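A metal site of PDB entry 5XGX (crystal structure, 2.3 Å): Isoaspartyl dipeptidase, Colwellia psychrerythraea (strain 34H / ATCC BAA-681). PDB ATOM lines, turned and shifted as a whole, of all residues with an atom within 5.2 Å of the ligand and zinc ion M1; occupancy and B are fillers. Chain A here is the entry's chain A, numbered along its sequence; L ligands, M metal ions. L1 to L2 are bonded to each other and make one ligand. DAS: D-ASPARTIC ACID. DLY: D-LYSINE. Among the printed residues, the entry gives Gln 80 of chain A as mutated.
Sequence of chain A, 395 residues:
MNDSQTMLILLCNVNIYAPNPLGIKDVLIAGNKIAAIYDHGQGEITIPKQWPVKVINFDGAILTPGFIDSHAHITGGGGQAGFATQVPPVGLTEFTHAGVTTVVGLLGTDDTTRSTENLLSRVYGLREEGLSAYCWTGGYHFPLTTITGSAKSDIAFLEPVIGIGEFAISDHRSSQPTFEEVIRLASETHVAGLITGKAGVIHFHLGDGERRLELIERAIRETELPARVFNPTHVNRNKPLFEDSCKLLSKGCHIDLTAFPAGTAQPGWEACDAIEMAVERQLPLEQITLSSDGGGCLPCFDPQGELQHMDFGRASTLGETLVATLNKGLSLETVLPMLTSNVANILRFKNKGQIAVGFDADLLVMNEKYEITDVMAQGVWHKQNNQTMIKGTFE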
ATOM      1  N   HIS A  71      17.147  15.832  31.234  1.00  0.00           N
ATOM      2  CA  HIS A  71      18.341  16.364  30.586  1.00  0.00           C
ATOM      3  C   HIS A  71      18.148  16.526  29.083  1.00  0.00           C
ATOM      4  O   HIS A  71      18.504  15.652  28.319  1.00  0.00           O
ATOM      5  CB  HIS A  71      19.479  15.432  30.900  1.00  0.00           C
ATOM      6  CG  HIS A  71      20.832  15.998  30.624  1.00  0.00           C
ATOM      7  ND1 HIS A  71      21.771  16.183  31.604  1.00  0.00           N
ATOM      8  CD2 HIS A  71      21.438  16.346  29.461  1.00  0.00           C
ATOM      9  CE1 HIS A  71      22.901  16.646  31.066  1.00  0.00           C
ATOM     10  NE2 HIS A  71      22.710  16.769  29.778  1.00  0.00           N
ATOM     11  N   HIS A  73      18.551  19.442  25.796  1.00  0.00           N
ATOM     12  CA  HIS A  73      18.924  20.764  25.290  1.00  0.00           C
ATOM     13  C   HIS A  73      17.850  21.266  24.352  1.00  0.00           C
ATOM     14  O   HIS A  73      17.940  21.099  23.126  1.00  0.00           O
ATOM     15  CB  HIS A  73      20.242  20.682  24.573  1.00  0.00           C
ATOM     16  CG  HIS A  73      21.347  20.310  25.501  1.00  0.00           C
ATOM     17  ND1 HIS A  73      22.017  21.253  26.254  1.00  0.00           N
ATOM     18  CD2 HIS A  73      21.834  19.109  25.875  1.00  0.00           C
ATOM     19  CE1 HIS A  73      22.923  20.645  26.995  1.00  0.00           C
ATOM     20  NE2 HIS A  73      22.836  19.346  26.768  1.00  0.00           N
ATOM     21  N   GLY A  77      21.907  22.130  21.636  1.00  0.00           N
ATOM     22  CA  GLY A  77      23.221  22.295  22.263  1.00  0.00           C
ATOM     23  C   GLY A  77      24.280  22.584  21.213  1.00  0.00           C
ATOM     24  O   GLY A  77      24.086  23.380  20.293  1.00  0.00           O
ATOM     25  N   GLY A  78      25.408  21.887  21.327  1.00  0.00           N
ATOM     26  CA  GLY A  78      26.480  22.018  20.393  1.00  0.00           C
ATOM     27  C   GLY A  78      27.235  23.295  20.566  1.00  0.00           C
ATOM     28  O   GLY A  78      27.289  23.856  21.659  1.00  0.00           O
ATOM     29  N   GLN A  80      30.540  23.335  19.998  1.00  0.00           N
ATOM     30  CA  GLN A  80      31.872  22.957  20.506  1.00  0.00           C
ATOM     31  C   GLN A  80      32.879  22.612  19.440  1.00  0.00           C
ATOM     32  O   GLN A  80      33.969  22.130  19.778  1.00  0.00           O
ATOM     33  CB  GLN A  80      31.765  21.752  21.384  1.00  0.00           C
ATOM     34  CG  GLN A  80      30.645  21.858  22.356  1.00  0.00           C
ATOM     35  CD  GLN A  80      30.537  20.605  23.131  1.00  0.00           C
ATOM     36  OE1 GLN A  80      31.560  20.050  23.549  1.00  0.00           O
ATOM     37  NE2 GLN A  80      29.307  20.110  23.297  1.00  0.00           N
ATOM     38  N   GLY A 108      24.434  23.634  28.123  1.00  0.00           N
ATOM     39  CA  GLY A 108      25.623  22.863  28.408  1.00  0.00           C
ATOM     40  C   GLY A 108      26.896  23.652  28.235  1.00  0.00           C
ATOM     41  O   GLY A 108      27.127  24.649  28.943  1.00  0.00           O
ATOM     42  N   THR A 109      27.751  23.166  27.339  1.00  0.00           N
ATOM     43  CA  THR A 109      29.075  23.731  27.146  1.00  0.00           C
ATOM     44  C   THR A 109      28.974  25.175  26.707  1.00  0.00           C
ATOM     45  O   THR A 109      29.695  26.014  27.193  1.00  0.00           O
ATOM     46  CB  THR A 109      29.907  22.973  26.099  1.00  0.00           C
ATOM     47  OG1 THR A 109      29.917  21.551  26.387  1.00  0.00           O
ATOM     48  CG2 THR A 109      31.361  23.462  26.128  1.00  0.00           C
ATOM     49  N   ASP A 110      28.098  25.462  25.736  1.00  0.00           N
ATOM     50  CA  ASP A 110      27.944  26.816  25.237  1.00  0.00           C
ATOM     51  C   ASP A 110      26.864  27.495  26.070  1.00  0.00           C
ATOM     52  O   ASP A 110      25.680  27.475  25.734  1.00  0.00           O
ATOM     53  CB  ASP A 110      27.645  26.866  23.730  1.00  0.00           C
ATOM     54  CG  ASP A 110      27.483  28.287  23.191  1.00  0.00           C
ATOM     55  OD1 ASP A 110      27.842  29.261  23.905  1.00  0.00           O
ATOM     56  OD2 ASP A 110      26.976  28.413  22.035  1.00  0.00           O
ATOM     57  N   TYR A 140      27.305  24.924  32.338  1.00  0.00           N
ATOM     58  CA  TYR A 140      28.587  24.259  32.682  1.00  0.00           C
ATOM     59  C   TYR A 140      29.418  25.081  33.611  1.00  0.00           C
ATOM     60  O   TYR A 140      30.181  24.498  34.414  1.00  0.00           O
ATOM     61  CB  TYR A 140      29.533  24.036  31.478  1.00  0.00           C
ATOM     62  CG  TYR A 140      29.560  22.689  30.761  1.00  0.00           C
ATOM     63  CD1 TYR A 140      28.412  21.965  30.551  1.00  0.00           C
ATOM     64  CD2 TYR A 140      30.736  22.183  30.216  1.00  0.00           C
ATOM     65  CE1 TYR A 140      28.429  20.760  29.830  1.00  0.00           C
ATOM     66  CE2 TYR A 140      30.783  20.954  29.534  1.00  0.00           C
ATOM     67  CZ  TYR A 140      29.625  20.267  29.305  1.00  0.00           C
ATOM     68  OH  TYR A 140      29.603  19.076  28.563  1.00  0.00           O
ATOM     69  N   GLU A 166      23.292  21.419  34.195  1.00  0.00           N
ATOM     70  CA  GLU A 166      24.487  20.842  33.741  1.00  0.00           C
ATOM     71  C   GLU A 166      25.756  21.579  34.122  1.00  0.00           C
ATOM     72  O   GLU A 166      26.500  22.024  33.250  1.00  0.00           O
ATOM     73  CB  GLU A 166      24.280  20.429  32.318  1.00  0.00           C
ATOM     74  CG  GLU A 166      25.498  20.154  31.567  1.00  0.00           C
ATOM     75  CD  GLU A 166      25.296  19.069  30.629  1.00  0.00           C
ATOM     76  OE1 GLU A 166      24.589  19.349  29.662  1.00  0.00           O
ATOM     77  OE2 GLU A 166      25.874  17.977  30.855  1.00  0.00           O
ATOM     78  N   ASP A 171      36.070  17.542  33.982  1.00  0.00           N
ATOM     79  CA  ASP A 171      35.954  17.690  32.520  1.00  0.00           C
ATOM     80  C   ASP A 171      36.884  18.800  32.040  1.00  0.00           C
ATOM     81  O   ASP A 171      36.987  19.883  32.681  1.00  0.00           O
ATOM     82  CB  ASP A 171      34.527  18.030  32.166  1.00  0.00           C
ATOM     83  CG  ASP A 171      34.217  17.867  30.664  1.00  0.00           C
ATOM     84  OD1 ASP A 171      34.736  18.698  29.891  1.00  0.00           O
ATOM     85  OD2 ASP A 171      33.465  16.913  30.259  1.00  0.00           O
ATOM     86  N   ARG A 173      36.379  20.815  29.746  1.00  0.00           N
ATOM     87  CA  ARG A 173      35.586  22.036  29.474  1.00  0.00           C
ATOM     88  C   ARG A 173      34.972  22.706  30.698  1.00  0.00           C
ATOM     89  O   ARG A 173      34.201  23.669  30.551  1.00  0.00           O
ATOM     90  CB  ARG A 173      34.488  21.764  28.528  1.00  0.00           C
ATOM     91  CG  ARG A 173      34.983  21.320  27.179  1.00  0.00           C
ATOM     92  CD  ARG A 173      34.689  19.879  27.003  1.00  0.00           C
ATOM     93  NE  ARG A 173      33.415  19.585  26.412  1.00  0.00           N
ATOM     94  CZ  ARG A 173      32.698  18.485  26.611  1.00  0.00           C
ATOM     95  NH1 ARG A 173      31.587  18.328  25.901  1.00  0.00           N
ATOM     96  NH2 ARG A 173      33.037  17.575  27.528  1.00  0.00           N
ATOM     97  N   HIS A 205      27.198  17.809  35.289  1.00  0.00           N
ATOM     98  CA  HIS A 205      27.826  17.149  34.133  1.00  0.00           C
ATOM     99  C   HIS A 205      29.141  16.554  34.599  1.00  0.00           C
ATOM    100  O   HIS A 205      29.954  17.240  35.179  1.00  0.00           O
ATOM    101  CB  HIS A 205      28.087  18.119  32.987  1.00  0.00           C
ATOM    102  CG  HIS A 205      29.096  17.634  31.988  1.00  0.00           C
ATOM    103  ND1 HIS A 205      28.729  17.031  30.804  1.00  0.00           N
ATOM    104  CD2 HIS A 205      30.453  17.660  31.992  1.00  0.00           C
ATOM    105  CE1 HIS A 205      29.818  16.709  30.119  1.00  0.00           C
ATOM    106  NE2 HIS A 205      30.878  17.093  30.809  1.00  0.00           N
ATOM    107  N   THR A 233      25.224  13.202  36.358  1.00  0.00           N
ATOM    108  CA  THR A 233      24.751  12.583  35.143  1.00  0.00           C
ATOM    109  C   THR A 233      25.934  12.113  34.321  1.00  0.00           C
ATOM    110  O   THR A 233      27.060  12.427  34.666  1.00  0.00           O
ATOM    111  CB  THR A 233      23.863  13.550  34.352  1.00  0.00           C
ATOM    112  OG1 THR A 233      23.099  12.820  33.374  1.00  0.00           O
ATOM    113  CG2 THR A 233      24.692  14.658  33.669  1.00  0.00           C
ATOM    114  N   HIS A 234      25.650  11.326  33.260  1.00  0.00           N
ATOM    115  CA  HIS A 234      26.620  10.696  32.371  1.00  0.00           C
ATOM    116  C   HIS A 234      27.443   9.667  33.094  1.00  0.00           C
ATOM    117  O   HIS A 234      28.578   9.365  32.714  1.00  0.00           O
ATOM    118  CB  HIS A 234      27.578  11.694  31.712  1.00  0.00           C
ATOM    119  CG  HIS A 234      26.936  12.892  31.111  1.00  0.00           C
ATOM    120  ND1 HIS A 234      25.799  12.837  30.348  1.00  0.00           N
ATOM    121  CD2 HIS A 234      27.333  14.191  31.077  1.00  0.00           C
ATOM    122  CE1 HIS A 234      25.483  14.043  29.926  1.00  0.00           C
ATOM    123  NE2 HIS A 234      26.391  14.887  30.367  1.00  0.00           N
ATOM    124  N   ARG A 237      29.455   7.043  31.436  1.00  0.00           N
ATOM    125  CA  ARG A 237      30.335   7.451  30.302  1.00  0.00           C
ATOM    126  C   ARG A 237      31.695   6.787  30.239  1.00  0.00           C
ATOM    127  O   ARG A 237      32.290   6.681  29.147  1.00  0.00           O
ATOM    128  CB  ARG A 237      30.560   9.006  30.263  1.00  0.00           C
ATOM    129  CG  ARG A 237      31.390   9.570  31.393  1.00  0.00           C
ATOM    130  CD  ARG A 237      31.520  11.086  31.343  1.00  0.00           C
ATOM    131  NE  ARG A 237      32.249  11.429  30.130  1.00  0.00           N
ATOM    132  CZ  ARG A 237      31.884  12.322  29.241  1.00  0.00           C
ATOM    133  NH1 ARG A 237      30.830  13.097  29.424  1.00  0.00           N
ATOM    134  NH2 ARG A 237      32.651  12.506  28.180  1.00  0.00           N
ATOM    135  N   THR A 258      23.043   8.330  30.975  1.00  0.00           N
ATOM    136  CA  THR A 258      22.719   8.909  29.688  1.00  0.00           C
ATOM    137  C   THR A 258      22.449   7.761  28.706  1.00  0.00           C
ATOM    138  O   THR A 258      23.277   6.853  28.543  1.00  0.00           O
ATOM    139  CB  THR A 258      23.863   9.821  29.232  1.00  0.00           C
ATOM    140  OG1 THR A 258      24.040  10.860  30.196  1.00  0.00           O
ATOM    141  CG2 THR A 258      23.531  10.452  27.903  1.00  0.00           C
ATOM    142  N   PHE A 260      22.882   6.873  25.599  1.00  0.00           N
ATOM    143  CA  PHE A 260      23.692   7.085  24.390  1.00  0.00           C
ATOM    144  C   PHE A 260      23.080   6.318  23.246  1.00  0.00           C
ATOM    145  O   PHE A 260      22.639   5.175  23.437  1.00  0.00           O
ATOM    146  CB  PHE A 260      25.144   6.583  24.555  1.00  0.00           C
ATOM    147  CG  PHE A 260      25.901   7.284  25.633  1.00  0.00           C
ATOM    148  CD1 PHE A 260      26.185   8.627  25.514  1.00  0.00           C
ATOM    149  CD2 PHE A 260      26.304   6.606  26.790  1.00  0.00           C
ATOM    150  CE1 PHE A 260      26.848   9.308  26.516  1.00  0.00           C
ATOM    151  CE2 PHE A 260      26.977   7.287  27.801  1.00  0.00           C
ATOM    152  CZ  PHE A 260      27.259   8.639  27.654  1.00  0.00           C
ATOM    153  N   THR A 264      27.493   3.600  20.670  1.00  0.00           N
ATOM    154  CA  THR A 264      28.293   4.854  20.814  1.00  0.00           C
ATOM    155  C   THR A 264      28.801   5.149  22.283  1.00  0.00           C
ATOM    156  O   THR A 264      29.548   6.136  22.537  1.00  0.00           O
ATOM    157  CB  THR A 264      27.507   6.079  20.233  1.00  0.00           C
ATOM    158  OG1 THR A 264      26.526   6.539  21.201  1.00  0.00           O
ATOM    159  CG2 THR A 264      26.817   5.727  18.834  1.00  0.00           C
ATOM    160  N   GLN A 266      31.107   4.370  24.005  1.00  0.00           N
ATOM    161  CA  GLN A 266      32.340   5.151  24.082  1.00  0.00           C
ATOM    162  C   GLN A 266      33.191   4.049  24.670  1.00  0.00           C
ATOM    163  O   GLN A 266      33.014   2.900  24.201  1.00  0.00           O
ATOM    164  CB  GLN A 266      32.068   6.440  24.947  1.00  0.00           C
ATOM    165  CG  GLN A 266      32.740   7.766  24.555  1.00  0.00           C
ATOM    166  CD  GLN A 266      32.438   8.901  25.551  1.00  0.00           C
ATOM    167  OE1 GLN A 266      31.660   8.724  26.520  1.00  0.00           O
ATOM    168  NE2 GLN A 266      33.054  10.077  25.309  1.00  0.00           N
ATOM    169  N   ASP A 293      19.701  13.323  26.871  1.00  0.00           N
ATOM    170  CA  ASP A 293      20.592  14.331  26.316  1.00  0.00           C
ATOM    171  C   ASP A 293      20.137  14.840  24.939  1.00  0.00           C
ATOM    172  O   ASP A 293      20.961  15.200  24.104  1.00  0.00           O
ATOM    173  CB  ASP A 293      22.021  13.788  26.276  1.00  0.00           C
ATOM    174  CG  ASP A 293      23.061  14.864  26.374  1.00  0.00           C
ATOM    175  OD1 ASP A 293      22.689  16.059  26.407  1.00  0.00           O
ATOM    176  OD2 ASP A 293      24.259  14.501  26.444  1.00  0.00           O
ATOM    177  N   GLY A 295      19.052  16.910  21.796  1.00  0.00           N
ATOM    178  CA  GLY A 295      19.581  18.148  21.274  1.00  0.00           C
ATOM    179  C   GLY A 295      21.058  18.425  21.572  1.00  0.00           C
ATOM    180  O   GLY A 295      21.594  19.413  21.067  1.00  0.00           O
ATOM    181  N   GLY A 296      21.709  17.582  22.363  1.00  0.00           N
ATOM    182  CA  GLY A 296      23.108  17.731  22.710  1.00  0.00           C
ATOM    183  C   GLY A 296      23.943  17.147  21.604  1.00  0.00           C
ATOM    184  O   GLY A 296      23.448  16.358  20.813  1.00  0.00           O
ATOM    185  N   CYS A 297      25.193  17.580  21.518  1.00  0.00           N
ATOM    186  CA  CYS A 297      26.210  16.880  20.732  1.00  0.00           C
ATOM    187  C   CYS A 297      26.989  15.978  21.704  1.00  0.00           C
ATOM    188  O   CYS A 297      27.169  16.333  22.874  1.00  0.00           O
ATOM    189  CB  CYS A 297      27.136  17.860  20.014  1.00  0.00           C
ATOM    190  SG  CYS A 297      28.299  18.691  21.115  1.00  0.00           S
ATOM    191  N   LEU A 298      27.422  14.823  21.211  1.00  0.00           N
ATOM    192  CA  LEU A 298      28.199  13.824  21.976  1.00  0.00           C
ATOM    193  C   LEU A 298      29.607  13.705  21.338  1.00  0.00           C
ATOM    194  O   LEU A 298      29.792  12.960  20.376  1.00  0.00           O
ATOM    195  CB  LEU A 298      27.454  12.470  21.967  1.00  0.00           C
ATOM    196  CG  LEU A 298      25.957  12.464  22.343  1.00  0.00           C
ATOM    197  CD1 LEU A 298      25.410  11.039  22.359  1.00  0.00           C
ATOM    198  CD2 LEU A 298      25.661  13.169  23.662  1.00  0.00           C
ATOM    199  N   PRO A 299      30.601  14.498  21.840  1.00  0.00           N
ATOM    200  CA  PRO A 299      31.927  14.606  21.152  1.00  0.00           C
ATOM    201  C   PRO A 299      32.938  13.426  21.304  1.00  0.00           C
ATOM    202  O   PRO A 299      33.048  12.805  22.373  1.00  0.00           O
ATOM    203  CB  PRO A 299      32.499  15.930  21.710  1.00  0.00           C
ATOM    204  CG  PRO A 299      31.819  16.141  23.023  1.00  0.00           C
ATOM    205  CD  PRO A 299      30.455  15.498  22.923  1.00  0.00           C
HETATM  206  N   DAS L   1      28.090  19.632  25.905  1.00  0.00           N
HETATM  207  CA  DAS L   1      26.618  19.671  25.830  1.00  0.00           C
HETATM  208  C   DAS L   1      26.156  20.545  24.587  1.00  0.00           C
HETATM  209  O   DAS L   1      25.985  20.018  23.445  1.00  0.00           O
HETATM  210  CB  DAS L   1      26.079  18.233  25.742  1.00  0.00           C
HETATM  211  CG  DAS L   1      26.922  17.279  26.519  1.00  0.00           C
HETATM  212  OD1 DAS L   1      27.154  17.403  27.751  1.00  0.00           O
HETATM  213  OXT DAS L   1      25.933  21.731  24.813  1.00  0.00           O
HETATM  214  N   DLY L   2      27.428  16.259  25.713  1.00  0.00           N
HETATM  215  CA  DLY L   2      28.330  15.169  26.090  1.00  0.00           C
HETATM  216  C   DLY L   2      29.712  15.756  26.542  1.00  0.00           C
HETATM  217  O   DLY L   2      30.693  14.969  26.645  1.00  0.00           O
HETATM  218  CB  DLY L   2      27.758  14.227  27.239  1.00  0.00           C
HETATM  219  CG  DLY L   2      27.710  12.678  26.867  1.00  0.00           C
HETATM  220  CD  DLY L   2      29.138  12.011  26.523  1.00  0.00           C
HETATM  221  CE  DLY L   2      29.511  12.079  25.000  1.00  0.00           C
HETATM  222  NZ  DLY L   2      30.111  10.814  24.553  1.00  0.00           N
HETATM  223  OXT DLY L   2      29.730  16.984  26.737  1.00  0.00           O
HETATM  224 ZN    ZN M   1      26.927  16.876  29.862  1.00  0.00          ZN
HETATM  225 ZN    ZN M   2      24.311  17.278  28.066  1.00  0.00          ZN
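The backbone NH (N) of Gly 78 lies within hydrogen-bond range of an oxygen (O) of DAS L1 (2.9 Å).
The side-chain hydroxyl (OH) of Tyr 140 lies within hydrogen-bond range of an oxygen (OXT) of DLY L2 (2.8 Å).
The guanidinium group of Arg 173 lies within salt-bridge range of an oxygen (OXT) of DLY L2 (2.4 Å).
The guanidinium group (NH1) of Arg 237 is in salt-bridge range of an oxygen (O) of DLY L2 (3.4 Å).
The side-chain amide nitrogen of Gln 80 sits close to a nitrogen (N) of DAS L1 (2.9 Å).
An oxygen (O) of DAS L1 sits at hydrogen-bond distance from the side-chain sulfur (SG) of Cys 297.
OG1 of Thr 109 lies within hydrogen-bond range of N of DAS L1 (2.7 Å).
The side-chain amide nitrogen (NE2) of Gln 266 sits close to a nitrogen (NZ) of DLY L2 (3.1 Å).
O of DAS L1 lies within hydrogen-bond range of N of Cys 297 (3.2 Å).
The backbone carbonyl oxygen (O) of Cys 297 lies within hydrogen-bond range of a nitrogen (N) of DLY L2, 2.9 Å away.
N of Thr 109 is in hydrogen-bond range of OXT of DAS L1 (3.4 Å).
The side-chain carboxylate (OE1) of Glu 166 lies within hydrogen-bond range of a ring nitrogen (NE2) of His 73, 3.4 Å away.
The side-chain carboxylate (OD1) of Asp 293 lies close to a ring nitrogen (NE2) of His 73 (3.3 Å).
The side-chain hydroxyl (OG1) of Thr 109 sits close to the side-chain hydroxyl (OH) of Tyr 140.
The backbone carbonyl oxygen of Glu 166 sits close to the backbone NH of Tyr 140 (3.1 Å).
The guanidinium group (NH1) of Arg 173 lies within hydrogen-bond range of the side-chain amide oxygen (OE1) of Gln 80 (2.9 Å).
The backbone carbonyl oxygen of Gly 295 sits at hydrogen-bond distance from the backbone NH of Gly 77, 2.8 Å away.
A ring nitrogen (NE2) of His 205 sits close to the side-chain hydroxyl of Tyr 140, 3.3 Å away.
NH1 of Arg 173 lies within hydrogen-bond range of OH of Tyr 140 (3.4 Å).
Merely in contact with the ligand: His 73 (3.6 Å), Gly 77 (3.8 Å), Gly 108 (3.8 Å), Phe 260 (3.5 Å), Asp 293 (3.6 Å), Gly 296 (3.7 Å), Leu 298 (3.7 Å) and Pro 299 (3.7 Å).
Within 4 Å of the ligand: His 73, Gly 77, Gly 78, Gln 80, Gly 108, Thr 109, Tyr 140, Glu 166, Arg 173, His 205, His 234, Arg 237, Phe 260, Gln 266, Asp 293, Gly 296, Cys 297, Leu 298 and Pro 299.
The nearest printed residue that does not touch the ligand is Asp 110 (4.4 Å).
Tyr 140 touches zinc ion M1 (OH to ZN, 3.7 Å).
Within 4 Å of zinc ion M1: Tyr 140, Glu 166, His 205 and His 234.
Zinc ion M1 is bound by the side-chain carboxylate (OE2) of Glu 166 (1.8 Å), a ring nitrogen (ND1) of His 205 (2.0 Å), a ring nitrogen (NE2) of His 234 (2.1 Å) and an oxygen (OD1) of DAS L1 (2.2 Å).
Zinc ion M1 has four donor atoms within binding distance.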
